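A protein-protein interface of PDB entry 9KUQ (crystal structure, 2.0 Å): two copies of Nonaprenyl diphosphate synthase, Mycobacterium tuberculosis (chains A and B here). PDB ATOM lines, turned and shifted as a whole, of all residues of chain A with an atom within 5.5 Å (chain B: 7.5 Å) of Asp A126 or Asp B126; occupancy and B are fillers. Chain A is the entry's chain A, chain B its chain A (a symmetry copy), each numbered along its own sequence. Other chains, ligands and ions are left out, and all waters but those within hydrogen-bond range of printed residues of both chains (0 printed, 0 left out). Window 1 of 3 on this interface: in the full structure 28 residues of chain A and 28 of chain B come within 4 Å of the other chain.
The side-chain carboxylate (OD2) of Asp B126 lies within hydrogen-bond range of a ring nitrogen (ND1) of His A96 (2.7 Å).
The side-chain sulfur (SD) of Met B100 sits close to the backbone NH (N) of Leu A123.
OD2 of Asp A126 is in hydrogen-bond range of ND1 of His B96 (2.7 Å).
The backbone carbonyl oxygen of Ile A122 is in hydrogen-bond range of a ring nitrogen (NE2) of His A96 (2.9 Å).
O of Tyr A127 is in hydrogen-bond range of OG1 of Thr A131.
A ring nitrogen (NE2) of His B96 sits at hydrogen-bond distance from the backbone carbonyl oxygen of Ile B122 (2.9 Å).
A ring nitrogen (NE2) of His B96 lies within hydrogen-bond range of the backbone NH (N) of Asp B126 (3.5 Å).
OE1 of Gln B158 lies close to OD1 of Asp B97 (2.6 Å).
The backbone carbonyl oxygen of Tyr B127 is in hydrogen-bond range of the side-chain hydroxyl of Thr B131.
Among the printed residues, pairs that only touch across the chains: Leu A123 with Gln B158 (3.0 Å), His A96 with Ile B122 (3.0 Å), Ile A122 with His B96 (3.0 Å), Ile A122 with Ile B122 (3.0 Å), Phe A151 with Asp B126 (3.2 Å), Asp A126 with Phe B151 (3.2 Å), Tyr A127 with Ala B152 (3.4 Å), Val A155 with Leu B123 (3.5 Å), Leu A123 with Val B155 (3.5 Å), Tyr A127 with Val B155 (3.6 Å), Val A155 with Tyr B127 (3.6 Å), Asp A126 with Asp B126 (3.6 Å), Phe A151 with Ala B130 (3.6 Å), Ala A130 with Phe B151 (3.6 Å), Ile A122 with Met B100 (3.8 Å), Ala A130 with Ala B152 (3.9 Å), His A96 with His B96 (3.9 Å) and Val A155 with Met B44 (3.96 Å).
Of the printed residues of chain B, Asp A126 touches His B96, Asp B126 and Phe B151.
Printed residues of chain A within 4 Å of Asp B126: His A96 (2.7 Å), Asp A126 (3.6 Å) and Phe A151 (3.2 Å).
No residue of chain B comes within 4 Å of Gly A125.
Printed residues of chain A within 4 Å of Met B100: Ile A122 (3.8 Å) and Leu A123 (3.0 Å).
Printed residues of chain B within 4 Å of Val A155: Met B44 (3.96 Å), Leu B123 (3.5 Å) and Tyr B127 (3.6 Å).
Of the printed residues of chain A, Met B44 touches Val A155.
Of the printed residues of chain A, Phe B151 touches Asp A126 (3.2 Å) and Ala A130 (3.6 Å).
The nearest printed residue of chain A that does not touch Asp B126 is Leu A129 (4.01 Å).
The nearest printed residue of chain A that does not touch Ala B152 is Thr A131 (5.5 Å).
Printed residues of chain B that touch a printed residue of chain A: Met B44, His B96, Met B100, Ile B122, Leu B123, Asp B126, Tyr B127, Ala B130, Phe B151, Ala B152, Val B155 and Gln B158.
Along chain B the printed residues that touch a printed residue of chain A span positions 44 to 158.
Printed residues of chain A that touch a printed residue of chain B: His A96, Ile A122, Leu A123, Asp A126, Tyr A127, Ala A130, Phe A151 and Val A155.
Hydrophobic or aromatic side chains of chain A within 4 Å of the printed part of chain B: His A96, Ile A122, Leu A123, Tyr A127, Ala A130, Phe A151 and Val A155.
Along chain A the printed residues that touch a printed residue of chain B span positions 96 to 155.
Among the printed residues, 21 pairs touch across the chains.
His A96 touches Asp B126, and with the chains exchanged Asp A126 touches His B96.
Asp A126 touches Phe B151, and with the chains exchanged Phe A151 touches Asp B126.
Tyr A127 touches Val B155, and with the chains exchanged Val A155 touches Tyr B127.
Ala A130 touches Phe B151, and with the chains exchanged Phe A151 touches Ala B130.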
ATOM      1  N   HIS A  96      21.991  11.273  14.683  1.00  0.00           N
ATOM      2  CA  HIS A  96      23.283  11.340  13.974  1.00  0.00           C
ATOM      3  C   HIS A  96      23.028  11.824  12.539  1.00  0.00           C
ATOM      4  O   HIS A  96      23.860  12.588  11.997  1.00  0.00           O
ATOM      5  CB  HIS A  96      24.005  10.007  14.185  1.00  0.00           C
ATOM      6  CG  HIS A  96      24.578   9.927  15.558  1.00  0.00           C
ATOM      7  ND1 HIS A  96      25.728   9.234  15.842  1.00  0.00           N
ATOM      8  CD2 HIS A  96      24.189  10.512  16.713  1.00  0.00           C
ATOM      9  CE1 HIS A  96      26.030   9.385  17.117  1.00  0.00           C
ATOM     10  NE2 HIS A  96      25.072  10.140  17.684  1.00  0.00           N
ATOM     11  N   ALA A 121      24.383  16.577  20.045  1.00  0.00           N
ATOM     12  CA  ALA A 121      23.597  15.529  19.352  1.00  0.00           C
ATOM     13  C   ALA A 121      24.502  14.331  19.076  1.00  0.00           C
ATOM     14  O   ALA A 121      23.989  13.235  19.064  1.00  0.00           O
ATOM     15  CB  ALA A 121      22.959  16.053  18.086  1.00  0.00           C
ATOM     16  N   ILE A 122      25.803  14.543  18.886  1.00  0.00           N
ATOM     17  CA  ILE A 122      26.743  13.419  18.598  1.00  0.00           C
ATOM     18  C   ILE A 122      26.837  12.558  19.857  1.00  0.00           C
ATOM     19  O   ILE A 122      26.755  11.306  19.751  1.00  0.00           O
ATOM     20  CB  ILE A 122      28.113  13.920  18.109  1.00  0.00           C
ATOM     21  CG1 ILE A 122      27.935  14.922  16.968  1.00  0.00           C
ATOM     22  CG2 ILE A 122      28.990  12.756  17.689  1.00  0.00           C
ATOM     23  CD1 ILE A 122      26.881  14.476  15.992  1.00  0.00           C
ATOM     24  N   LEU A 123      26.957  13.200  21.014  1.00  0.00           N
ATOM     25  CA  LEU A 123      27.210  12.475  22.284  1.00  0.00           C
ATOM     26  C   LEU A 123      25.921  11.778  22.753  1.00  0.00           C
ATOM     27  O   LEU A 123      26.035  10.572  23.123  1.00  0.00           O
ATOM     28  CB  LEU A 123      27.844  13.418  23.313  1.00  0.00           C
ATOM     29  CG  LEU A 123      29.370  13.534  23.187  1.00  0.00           C
ATOM     30  CD1 LEU A 123      30.070  12.278  23.683  1.00  0.00           C
ATOM     31  CD2 LEU A 123      29.809  13.802  21.751  1.00  0.00           C
ATOM     32  N   ALA A 124      24.751  12.430  22.652  1.00  0.00           N
ATOM     33  CA  ALA A 124      23.456  11.849  23.088  1.00  0.00           C
ATOM     34  C   ALA A 124      23.209  10.537  22.336  1.00  0.00           C
ATOM     35  O   ALA A 124      23.183   9.464  22.970  1.00  0.00           O
ATOM     36  CB  ALA A 124      22.349  12.820  22.806  1.00  0.00           C
ATOM     37  N   GLY A 125      23.025  10.617  21.019  1.00  0.00           N
ATOM     38  CA  GLY A 125      22.970   9.421  20.163  1.00  0.00           C
ATOM     39  C   GLY A 125      24.003   8.415  20.615  1.00  0.00           C
ATOM     40  O   GLY A 125      23.642   7.242  20.715  1.00  0.00           O
ATOM     41  N   ASP A 126      25.235   8.861  20.888  1.00  0.00           N
ATOM     42  CA  ASP A 126      26.345   7.994  21.353  1.00  0.00           C
ATOM     43  C   ASP A 126      25.907   7.289  22.646  1.00  0.00           C
ATOM     44  O   ASP A 126      26.319   6.128  22.856  1.00  0.00           O
ATOM     45  CB  ASP A 126      27.648   8.775  21.529  1.00  0.00           C
ATOM     46  CG  ASP A 126      28.437   9.007  20.255  1.00  0.00           C
ATOM     47  OD1 ASP A 126      28.002   8.491  19.200  1.00  0.00           O
ATOM     48  OD2 ASP A 126      29.499   9.700  20.333  1.00  0.00           O
ATOM     49  N   TYR A 127      25.073   7.933  23.468  1.00  0.00           N
ATOM     50  CA  TYR A 127      24.575   7.365  24.742  1.00  0.00           C
ATOM     51  C   TYR A 127      23.543   6.303  24.391  1.00  0.00           C
ATOM     52  O   TYR A 127      23.779   5.113  24.739  1.00  0.00           O
ATOM     53  CB  TYR A 127      23.998   8.417  25.702  1.00  0.00           C
ATOM     54  CG  TYR A 127      23.988   7.947  27.141  1.00  0.00           C
ATOM     55  CD1 TYR A 127      25.130   8.021  27.936  1.00  0.00           C
ATOM     56  CD2 TYR A 127      22.854   7.394  27.709  1.00  0.00           C
ATOM     57  CE1 TYR A 127      25.149   7.572  29.255  1.00  0.00           C
ATOM     58  CE2 TYR A 127      22.855   6.929  29.020  1.00  0.00           C
ATOM     59  CZ  TYR A 127      24.006   7.009  29.795  1.00  0.00           C
ATOM     60  OH  TYR A 127      24.032   6.529  31.077  1.00  0.00           O
ATOM     61  N   LEU A 128      22.492   6.701  23.669  1.00  0.00           N
ATOM     62  CA  LEU A 128      21.444   5.756  23.226  1.00  0.00           C
ATOM     63  C   LEU A 128      22.121   4.470  22.743  1.00  0.00           C
ATOM     64  O   LEU A 128      21.577   3.411  23.102  1.00  0.00           O
ATOM     65  CB  LEU A 128      20.537   6.390  22.171  1.00  0.00           C
ATOM     66  CG  LEU A 128      19.343   7.149  22.736  1.00  0.00           C
ATOM     67  CD1 LEU A 128      18.690   8.026  21.689  1.00  0.00           C
ATOM     68  CD2 LEU A 128      18.308   6.198  23.305  1.00  0.00           C
ATOM     69  N   LEU A 129      23.283   4.556  22.068  1.00  0.00           N
ATOM     70  CA  LEU A 129      24.087   3.398  21.574  1.00  0.00           C
ATOM     71  C   LEU A 129      24.798   2.657  22.728  1.00  0.00           C
ATOM     72  O   LEU A 129      24.919   1.422  22.645  1.00  0.00           O
ATOM     73  CB  LEU A 129      25.112   3.869  20.536  1.00  0.00           C
ATOM     74  CG  LEU A 129      24.514   4.445  19.250  1.00  0.00           C
ATOM     75  CD1 LEU A 129      25.580   5.124  18.420  1.00  0.00           C
ATOM     76  CD2 LEU A 129      23.804   3.369  18.444  1.00  0.00           C
ATOM     77  N   ALA A 130      25.290   3.367  23.748  1.00  0.00           N
ATOM     78  CA  ALA A 130      25.962   2.739  24.911  1.00  0.00           C
ATOM     79  C   ALA A 130      24.956   1.861  25.681  1.00  0.00           C
ATOM     80  O   ALA A 130      25.261   0.683  25.951  1.00  0.00           O
ATOM     81  CB  ALA A 130      26.548   3.811  25.792  1.00  0.00           C
ATOM     82  N   THR A 131      23.822   2.473  25.994  1.00  0.00           N
ATOM     83  CA  THR A 131      22.591   1.991  26.662  1.00  0.00           C
ATOM     84  C   THR A 131      21.976   0.791  25.941  1.00  0.00           C
ATOM     85  O   THR A 131      21.756  -0.231  26.601  1.00  0.00           O
ATOM     86  CB  THR A 131      21.605   3.153  26.690  1.00  0.00           C
ATOM     87  OG1 THR A 131      22.424   4.228  27.149  1.00  0.00           O
ATOM     88  CG2 THR A 131      20.393   2.915  27.567  1.00  0.00           C
ATOM     89  N   PHE A 151      24.164  -2.925  13.417  1.00  0.00           N
ATOM     90  CA  PHE A 151      24.463  -1.473  13.515  1.00  0.00           C
ATOM     91  C   PHE A 151      25.453  -1.184  12.381  1.00  0.00           C
ATOM     92  O   PHE A 151      25.250  -0.184  11.704  1.00  0.00           O
ATOM     93  CB  PHE A 151      24.895  -1.060  14.922  1.00  0.00           C
ATOM     94  CG  PHE A 151      25.093   0.435  15.049  1.00  0.00           C
ATOM     95  CD1 PHE A 151      24.077   1.316  14.718  1.00  0.00           C
ATOM     96  CD2 PHE A 151      26.311   0.965  15.448  1.00  0.00           C
ATOM     97  CE1 PHE A 151      24.268   2.691  14.797  1.00  0.00           C
ATOM     98  CE2 PHE A 151      26.494   2.341  15.545  1.00  0.00           C
ATOM     99  CZ  PHE A 151      25.463   3.199  15.242  1.00  0.00           C
ATOM    100  N   VAL A 155      25.029   1.701   9.415  1.00  0.00           N
ATOM    101  CA  VAL A 155      25.980   2.810   9.191  1.00  0.00           C
ATOM    102  C   VAL A 155      26.277   2.857   7.690  1.00  0.00           C
ATOM    103  O   VAL A 155      25.945   3.897   7.064  1.00  0.00           O
ATOM    104  CB  VAL A 155      27.229   2.597  10.063  1.00  0.00           C
ATOM    105  CG1 VAL A 155      28.398   3.464   9.627  1.00  0.00           C
ATOM    106  CG2 VAL A 155      26.897   2.809  11.544  1.00  0.00           C
ATOM    107  N   MET B  44      32.911   3.350   3.383  1.00  0.00           N
ATOM    108  CA  MET B  44      33.478   3.581   4.751  1.00  0.00           C
ATOM    109  C   MET B  44      34.956   3.990   4.720  1.00  0.00           C
ATOM    110  O   MET B  44      35.353   4.811   5.591  1.00  0.00           O
ATOM    111  CB  MET B  44      33.409   2.289   5.575  1.00  0.00           C
ATOM    112  CG  MET B  44      32.003   1.823   5.862  1.00  0.00           C
ATOM    113  SD  MET B  44      31.078   3.102   6.740  1.00  0.00           S
ATOM    114  CE  MET B  44      32.310   3.634   7.936  1.00  0.00           C
ATOM    115  N   LEU B  48      36.982   6.016   7.813  1.00  0.00           N
ATOM    116  CA  LEU B  48      37.533   5.143   8.897  1.00  0.00           C
ATOM    117  C   LEU B  48      39.062   5.259   8.994  1.00  0.00           C
ATOM    118  O   LEU B  48      39.576   5.391  10.109  1.00  0.00           O
ATOM    119  CB  LEU B  48      37.152   3.686   8.611  1.00  0.00           C
ATOM    120  CG  LEU B  48      35.725   3.259   8.962  1.00  0.00           C
ATOM    121  CD1 LEU B  48      35.564   1.759   8.781  1.00  0.00           C
ATOM    122  CD2 LEU B  48      35.364   3.649  10.390  1.00  0.00           C
ATOM    123  N   ALA B  92      37.206   6.537  18.025  1.00  0.00           N
ATOM    124  CA  ALA B  92      35.799   6.900  17.782  1.00  0.00           C
ATOM    125  C   ALA B  92      35.424   8.191  18.520  1.00  0.00           C
ATOM    126  O   ALA B  92      34.616   8.972  17.968  1.00  0.00           O
ATOM    127  CB  ALA B  92      34.859   5.787  18.202  1.00  0.00           C
ATOM    128  N   THR B  93      35.848   8.344  19.774  1.00  0.00           N
ATOM    129  CA  THR B  93      35.511   9.543  20.592  1.00  0.00           C
ATOM    130  C   THR B  93      36.109  10.804  19.951  1.00  0.00           C
ATOM    131  O   THR B  93      35.439  11.860  19.987  1.00  0.00           O
ATOM    132  CB  THR B  93      35.989   9.427  22.037  1.00  0.00           C
ATOM    133  OG1 THR B  93      37.408   9.318  22.118  1.00  0.00           O
ATOM    134  CG2 THR B  93      35.357   8.238  22.711  1.00  0.00           C
ATOM    135  N   TYR B  95      36.651  11.468  16.659  1.00  0.00           N
ATOM    136  CA  TYR B  95      35.706  11.820  15.574  1.00  0.00           C
ATOM    137  C   TYR B  95      34.508  12.614  16.089  1.00  0.00           C
ATOM    138  O   TYR B  95      33.978  13.457  15.352  1.00  0.00           O
ATOM    139  CB  TYR B  95      35.045  10.598  14.923  1.00  0.00           C
ATOM    140  CG  TYR B  95      35.848   9.867  13.883  1.00  0.00           C
ATOM    141  CD1 TYR B  95      36.898   9.055  14.258  1.00  0.00           C
ATOM    142  CD2 TYR B  95      35.543   9.959  12.530  1.00  0.00           C
ATOM    143  CE1 TYR B  95      37.640   8.357  13.323  1.00  0.00           C
ATOM    144  CE2 TYR B  95      36.274   9.264  11.577  1.00  0.00           C
ATOM    145  CZ  TYR B  95      37.333   8.464  11.978  1.00  0.00           C
ATOM    146  OH  TYR B  95      38.099   7.770  11.088  1.00  0.00           O
ATOM    147  N   HIS B  96      33.962  12.234  17.239  1.00  0.00           N
ATOM    148  CA  HIS B  96      32.673  12.783  17.701  1.00  0.00           C
ATOM    149  C   HIS B  96      32.938  14.121  18.407  1.00  0.00           C
ATOM    150  O   HIS B  96      32.114  15.056  18.271  1.00  0.00           O
ATOM    151  CB  HIS B  96      31.938  11.678  18.465  1.00  0.00           C
ATOM    152  CG  HIS B  96      31.360  10.679  17.524  1.00  0.00           C
ATOM    153  ND1 HIS B  96      30.203   9.991  17.792  1.00  0.00           N
ATOM    154  CD2 HIS B  96      31.750  10.303  16.286  1.00  0.00           C
ATOM    155  CE1 HIS B  96      29.898   9.225  16.764  1.00  0.00           C
ATOM    156  NE2 HIS B  96      30.861   9.372  15.835  1.00  0.00           N
ATOM    157  N   ASP B  97      34.054  14.208  19.116  1.00  0.00           N
ATOM    158  CA  ASP B  97      34.502  15.440  19.820  1.00  0.00           C
ATOM    159  C   ASP B  97      34.676  16.535  18.769  1.00  0.00           C
ATOM    160  O   ASP B  97      34.067  17.635  18.945  1.00  0.00           O
ATOM    161  CB  ASP B  97      35.800  15.166  20.576  1.00  0.00           C
ATOM    162  CG  ASP B  97      35.582  14.546  21.949  1.00  0.00           C
ATOM    163  OD1 ASP B  97      34.411  14.483  22.397  1.00  0.00           O
ATOM    164  OD2 ASP B  97      36.584  14.167  22.573  1.00  0.00           O
ATOM    165  N   MET B 100      31.248  18.243  17.585  1.00  0.00           N
ATOM    166  CA  MET B 100      30.590  19.091  18.615  1.00  0.00           C
ATOM    167  C   MET B 100      31.493  20.268  19.008  1.00  0.00           C
ATOM    168  O   MET B 100      30.948  21.287  19.427  1.00  0.00           O
ATOM    169  CB  MET B 100      30.212  18.281  19.855  1.00  0.00           C
ATOM    170  CG  MET B 100      28.858  17.631  19.679  1.00  0.00           C
ATOM    171  SD  MET B 100      28.457  16.410  20.951  1.00  0.00           S
ATOM    172  CE  MET B 100      29.038  17.240  22.430  1.00  0.00           C
ATOM    173  N   VAL B 120      30.230  13.431   7.546  1.00  0.00           N
ATOM    174  CA  VAL B 120      30.325  11.940   7.618  1.00  0.00           C
ATOM    175  C   VAL B 120      31.200  11.482   8.803  1.00  0.00           C
ATOM    176  O   VAL B 120      31.430  10.255   8.925  1.00  0.00           O
ATOM    177  CB  VAL B 120      30.793  11.350   6.268  1.00  0.00           C
ATOM    178  CG1 VAL B 120      30.158  12.080   5.083  1.00  0.00           C
ATOM    179  CG2 VAL B 120      32.309  11.308   6.111  1.00  0.00           C
ATOM    180  N   ALA B 121      31.597  12.399   9.690  1.00  0.00           N
ATOM    181  CA  ALA B 121      32.377  12.112  10.917  1.00  0.00           C
ATOM    182  C   ALA B 121      31.462  11.442  11.940  1.00  0.00           C
ATOM    183  O   ALA B 121      31.967  10.652  12.706  1.00  0.00           O
ATOM    184  CB  ALA B 121      33.023  13.358  11.475  1.00  0.00           C
ATOM    185  N   ILE B 122      30.164  11.738  11.926  1.00  0.00           N
ATOM    186  CA  ILE B 122      29.215  11.131  12.906  1.00  0.00           C
ATOM    187  C   ILE B 122      29.110   9.640  12.588  1.00  0.00           C
ATOM    188  O   ILE B 122      29.180   8.805  13.529  1.00  0.00           O
ATOM    189  CB  ILE B 122      27.852  11.842  12.911  1.00  0.00           C
ATOM    190  CG1 ILE B 122      28.043  13.354  13.048  1.00  0.00           C
ATOM    191  CG2 ILE B 122      26.966  11.297  14.015  1.00  0.00           C
ATOM    192  CD1 ILE B 122      29.096  13.694  14.065  1.00  0.00           C
ATOM    193  N   LEU B 123      28.990   9.308  11.307  1.00  0.00           N
ATOM    194  CA  LEU B 123      28.727   7.910  10.886  1.00  0.00           C
ATOM    195  C   LEU B 123      30.008   7.070  11.032  1.00  0.00           C
ATOM    196  O   LEU B 123      29.882   5.943  11.595  1.00  0.00           O
ATOM    197  CB  LEU B 123      28.098   7.889   9.488  1.00  0.00           C
ATOM    198  CG  LEU B 123      26.573   8.073   9.494  1.00  0.00           C
ATOM    199  CD1 LEU B 123      25.861   6.828   9.999  1.00  0.00           C
ATOM    200  CD2 LEU B 123      26.142   9.261  10.348  1.00  0.00           C
ATOM    201  N   ALA B 124      31.185   7.602  10.659  1.00  0.00           N
ATOM    202  CA  ALA B 124      32.473   6.869  10.749  1.00  0.00           C
ATOM    203  C   ALA B 124      32.710   6.435  12.198  1.00  0.00           C
ATOM    204  O   ALA B 124      32.725   5.220  12.480  1.00  0.00           O
ATOM    205  CB  ALA B 124      33.590   7.757  10.288  1.00  0.00           C
ATOM    206  N   GLY B 125      32.900   7.400  13.099  1.00  0.00           N
ATOM    207  CA  GLY B 125      32.947   7.124  14.543  1.00  0.00           C
ATOM    208  C   GLY B 125      31.904   6.091  14.906  1.00  0.00           C
ATOM    209  O   GLY B 125      32.255   5.171  15.643  1.00  0.00           O
ATOM    210  N   ASP B 126      30.675   6.237  14.396  1.00  0.00           N
ATOM    211  CA  ASP B 126      29.555   5.298  14.654  1.00  0.00           C
ATOM    212  C   ASP B 126      29.983   3.893  14.205  1.00  0.00           C
ATOM    213  O   ASP B 126      29.560   2.911  14.852  1.00  0.00           O
ATOM    214  CB  ASP B 126      28.260   5.754  13.983  1.00  0.00           C
ATOM    215  CG  ASP B 126      27.477   6.808  14.743  1.00  0.00           C
ATOM    216  OD1 ASP B 126      27.911   7.158  15.864  1.00  0.00           O
ATOM    217  OD2 ASP B 126      26.420   7.265  14.205  1.00  0.00           O
ATOM    218  N   TYR B 127      30.820   3.785  13.168  1.00  0.00           N
ATOM    219  CA  TYR B 127      31.308   2.491  12.638  1.00  0.00           C
ATOM    220  C   TYR B 127      32.333   1.955  13.628  1.00  0.00           C
ATOM    221  O   TYR B 127      32.084   0.855  14.196  1.00  0.00           O
ATOM    222  CB  TYR B 127      31.891   2.586  11.221  1.00  0.00           C
ATOM    223  CG  TYR B 127      31.892   1.254  10.502  1.00  0.00           C
ATOM    224  CD1 TYR B 127      30.748   0.769   9.872  1.00  0.00           C
ATOM    225  CD2 TYR B 127      33.019   0.451  10.476  1.00  0.00           C
ATOM    226  CE1 TYR B 127      30.720  -0.466   9.226  1.00  0.00           C
ATOM    227  CE2 TYR B 127      33.010  -0.789   9.847  1.00  0.00           C
ATOM    228  CZ  TYR B 127      31.857  -1.256   9.226  1.00  0.00           C
ATOM    229  OH  TYR B 127      31.822  -2.487   8.629  1.00  0.00           O
ATOM    230  N   LEU B 128      33.389   2.732  13.880  1.00  0.00           N
ATOM    231  CA  LEU B 128      34.431   2.343  14.857  1.00  0.00           C
ATOM    232  C   LEU B 128      33.744   1.751  16.091  1.00  0.00           C
ATOM    233  O   LEU B 128      34.277   0.731  16.563  1.00  0.00           O
ATOM    234  CB  LEU B 128      35.347   3.522  15.188  1.00  0.00           C
ATOM    235  CG  LEU B 128      36.546   3.672  14.259  1.00  0.00           C
ATOM    236  CD1 LEU B 128      37.209   5.023  14.415  1.00  0.00           C
ATOM    237  CD2 LEU B 128      37.570   2.581  14.506  1.00  0.00           C
ATOM    238  N   LEU B 129      32.585   2.289  16.517  1.00  0.00           N
ATOM    239  CA  LEU B 129      31.772   1.798  17.670  1.00  0.00           C
ATOM    240  C   LEU B 129      31.052   0.472  17.343  1.00  0.00           C
ATOM    241  O   LEU B 129      30.919  -0.364  18.254  1.00  0.00           O
ATOM    242  CB  LEU B 129      30.755   2.863  18.093  1.00  0.00           C
ATOM    243  CG  LEU B 129      31.363   4.162  18.630  1.00  0.00           C
ATOM    244  CD1 LEU B 129      30.306   5.235  18.759  1.00  0.00           C
ATOM    245  CD2 LEU B 129      32.067   3.933  19.958  1.00  0.00           C
ATOM    246  N   ALA B 130      30.561   0.287  16.113  1.00  0.00           N
ATOM    247  CA  ALA B 130      29.880  -0.964  15.701  1.00  0.00           C
ATOM    248  C   ALA B 130      30.876  -2.139  15.753  1.00  0.00           C
ATOM    249  O   ALA B 130      30.560  -3.176  16.368  1.00  0.00           O
ATOM    250  CB  ALA B 130      29.300  -0.790  14.322  1.00  0.00           C
ATOM    251  N   THR B 131      32.014  -1.921  15.107  1.00  0.00           N
ATOM    252  CA  THR B 131      33.238  -2.742  14.960  1.00  0.00           C
ATOM    253  C   THR B 131      33.846  -3.119  16.312  1.00  0.00           C
ATOM    254  O   THR B 131      34.054  -4.317  16.539  1.00  0.00           O
ATOM    255  CB  THR B 131      34.235  -1.929  14.142  1.00  0.00           C
ATOM    256  OG1 THR B 131      33.423  -1.460  13.065  1.00  0.00           O
ATOM    257  CG2 THR B 131      35.441  -2.716  13.675  1.00  0.00           C
ATOM    258  N   ALA B 132      34.135  -2.124  17.144  1.00  0.00           N
ATOM    259  CA  ALA B 132      34.458  -2.296  18.577  1.00  0.00           C
ATOM    260  C   ALA B 132      33.494  -3.322  19.151  1.00  0.00           C
ATOM    261  O   ALA B 132      33.925  -4.217  19.873  1.00  0.00           O
ATOM    262  CB  ALA B 132      34.303  -0.995  19.344  1.00  0.00           C
ATOM    263  N   PHE B 151      31.669   2.844  27.938  1.00  0.00           N
ATOM    264  CA  PHE B 151      31.382   3.829  26.864  1.00  0.00           C
ATOM    265  C   PHE B 151      30.399   4.829  27.483  1.00  0.00           C
ATOM    266  O   PHE B 151      30.613   6.019  27.284  1.00  0.00           O
ATOM    267  CB  PHE B 151      30.949   3.163  25.559  1.00  0.00           C
ATOM    268  CG  PHE B 151      30.764   4.159  24.436  1.00  0.00           C
ATOM    269  CD1 PHE B 151      31.789   5.017  24.072  1.00  0.00           C
ATOM    270  CD2 PHE B 151      29.549   4.279  23.777  1.00  0.00           C
ATOM    271  CE1 PHE B 151      31.609   5.961  23.066  1.00  0.00           C
ATOM    272  CE2 PHE B 151      29.378   5.210  22.758  1.00  0.00           C
ATOM    273  CZ  PHE B 151      30.417   6.032  22.389  1.00  0.00           C
ATOM    274  N   ALA B 152      29.448   4.339  28.292  1.00  0.00           N
ATOM    275  CA  ALA B 152      28.374   5.103  28.964  1.00  0.00           C
ATOM    276  C   ALA B 152      28.974   6.177  29.873  1.00  0.00           C
ATOM    277  O   ALA B 152      28.459   7.311  29.896  1.00  0.00           O
ATOM    278  CB  ALA B 152      27.500   4.177  29.751  1.00  0.00           C
ATOM    279  N   VAL B 155      30.858   8.960  27.643  1.00  0.00           N
ATOM    280  CA  VAL B 155      29.918   9.926  27.039  1.00  0.00           C
ATOM    281  C   VAL B 155      29.627  10.998  28.091  1.00  0.00           C
ATOM    282  O   VAL B 155      29.970  12.180  27.829  1.00  0.00           O
ATOM    283  CB  VAL B 155      28.664   9.181  26.549  1.00  0.00           C
ATOM    284  CG1 VAL B 155      27.504  10.120  26.263  1.00  0.00           C
ATOM    285  CG2 VAL B 155      28.992   8.312  25.331  1.00  0.00           C
ATOM    286  N   GLN B 158      32.463  13.597  28.381  1.00  0.00           N
ATOM    287  CA  GLN B 158      32.442  14.554  27.241  1.00  0.00           C
ATOM    288  C   GLN B 158      31.215  15.467  27.415  1.00  0.00           C
ATOM    289  O   GLN B 158      31.365  16.708  27.314  1.00  0.00           O
ATOM    290  CB  GLN B 158      32.399  13.808  25.900  1.00  0.00           C
ATOM    291  CG  GLN B 158      33.696  13.094  25.525  1.00  0.00           C
ATOM    292  CD  GLN B 158      33.474  12.069  24.434  1.00  0.00           C
ATOM    293  OE1 GLN B 158      34.046  12.148  23.355  1.00  0.00           O
ATOM    294  NE2 GLN B 158      32.615  11.094  24.692  1.00  0.00           N
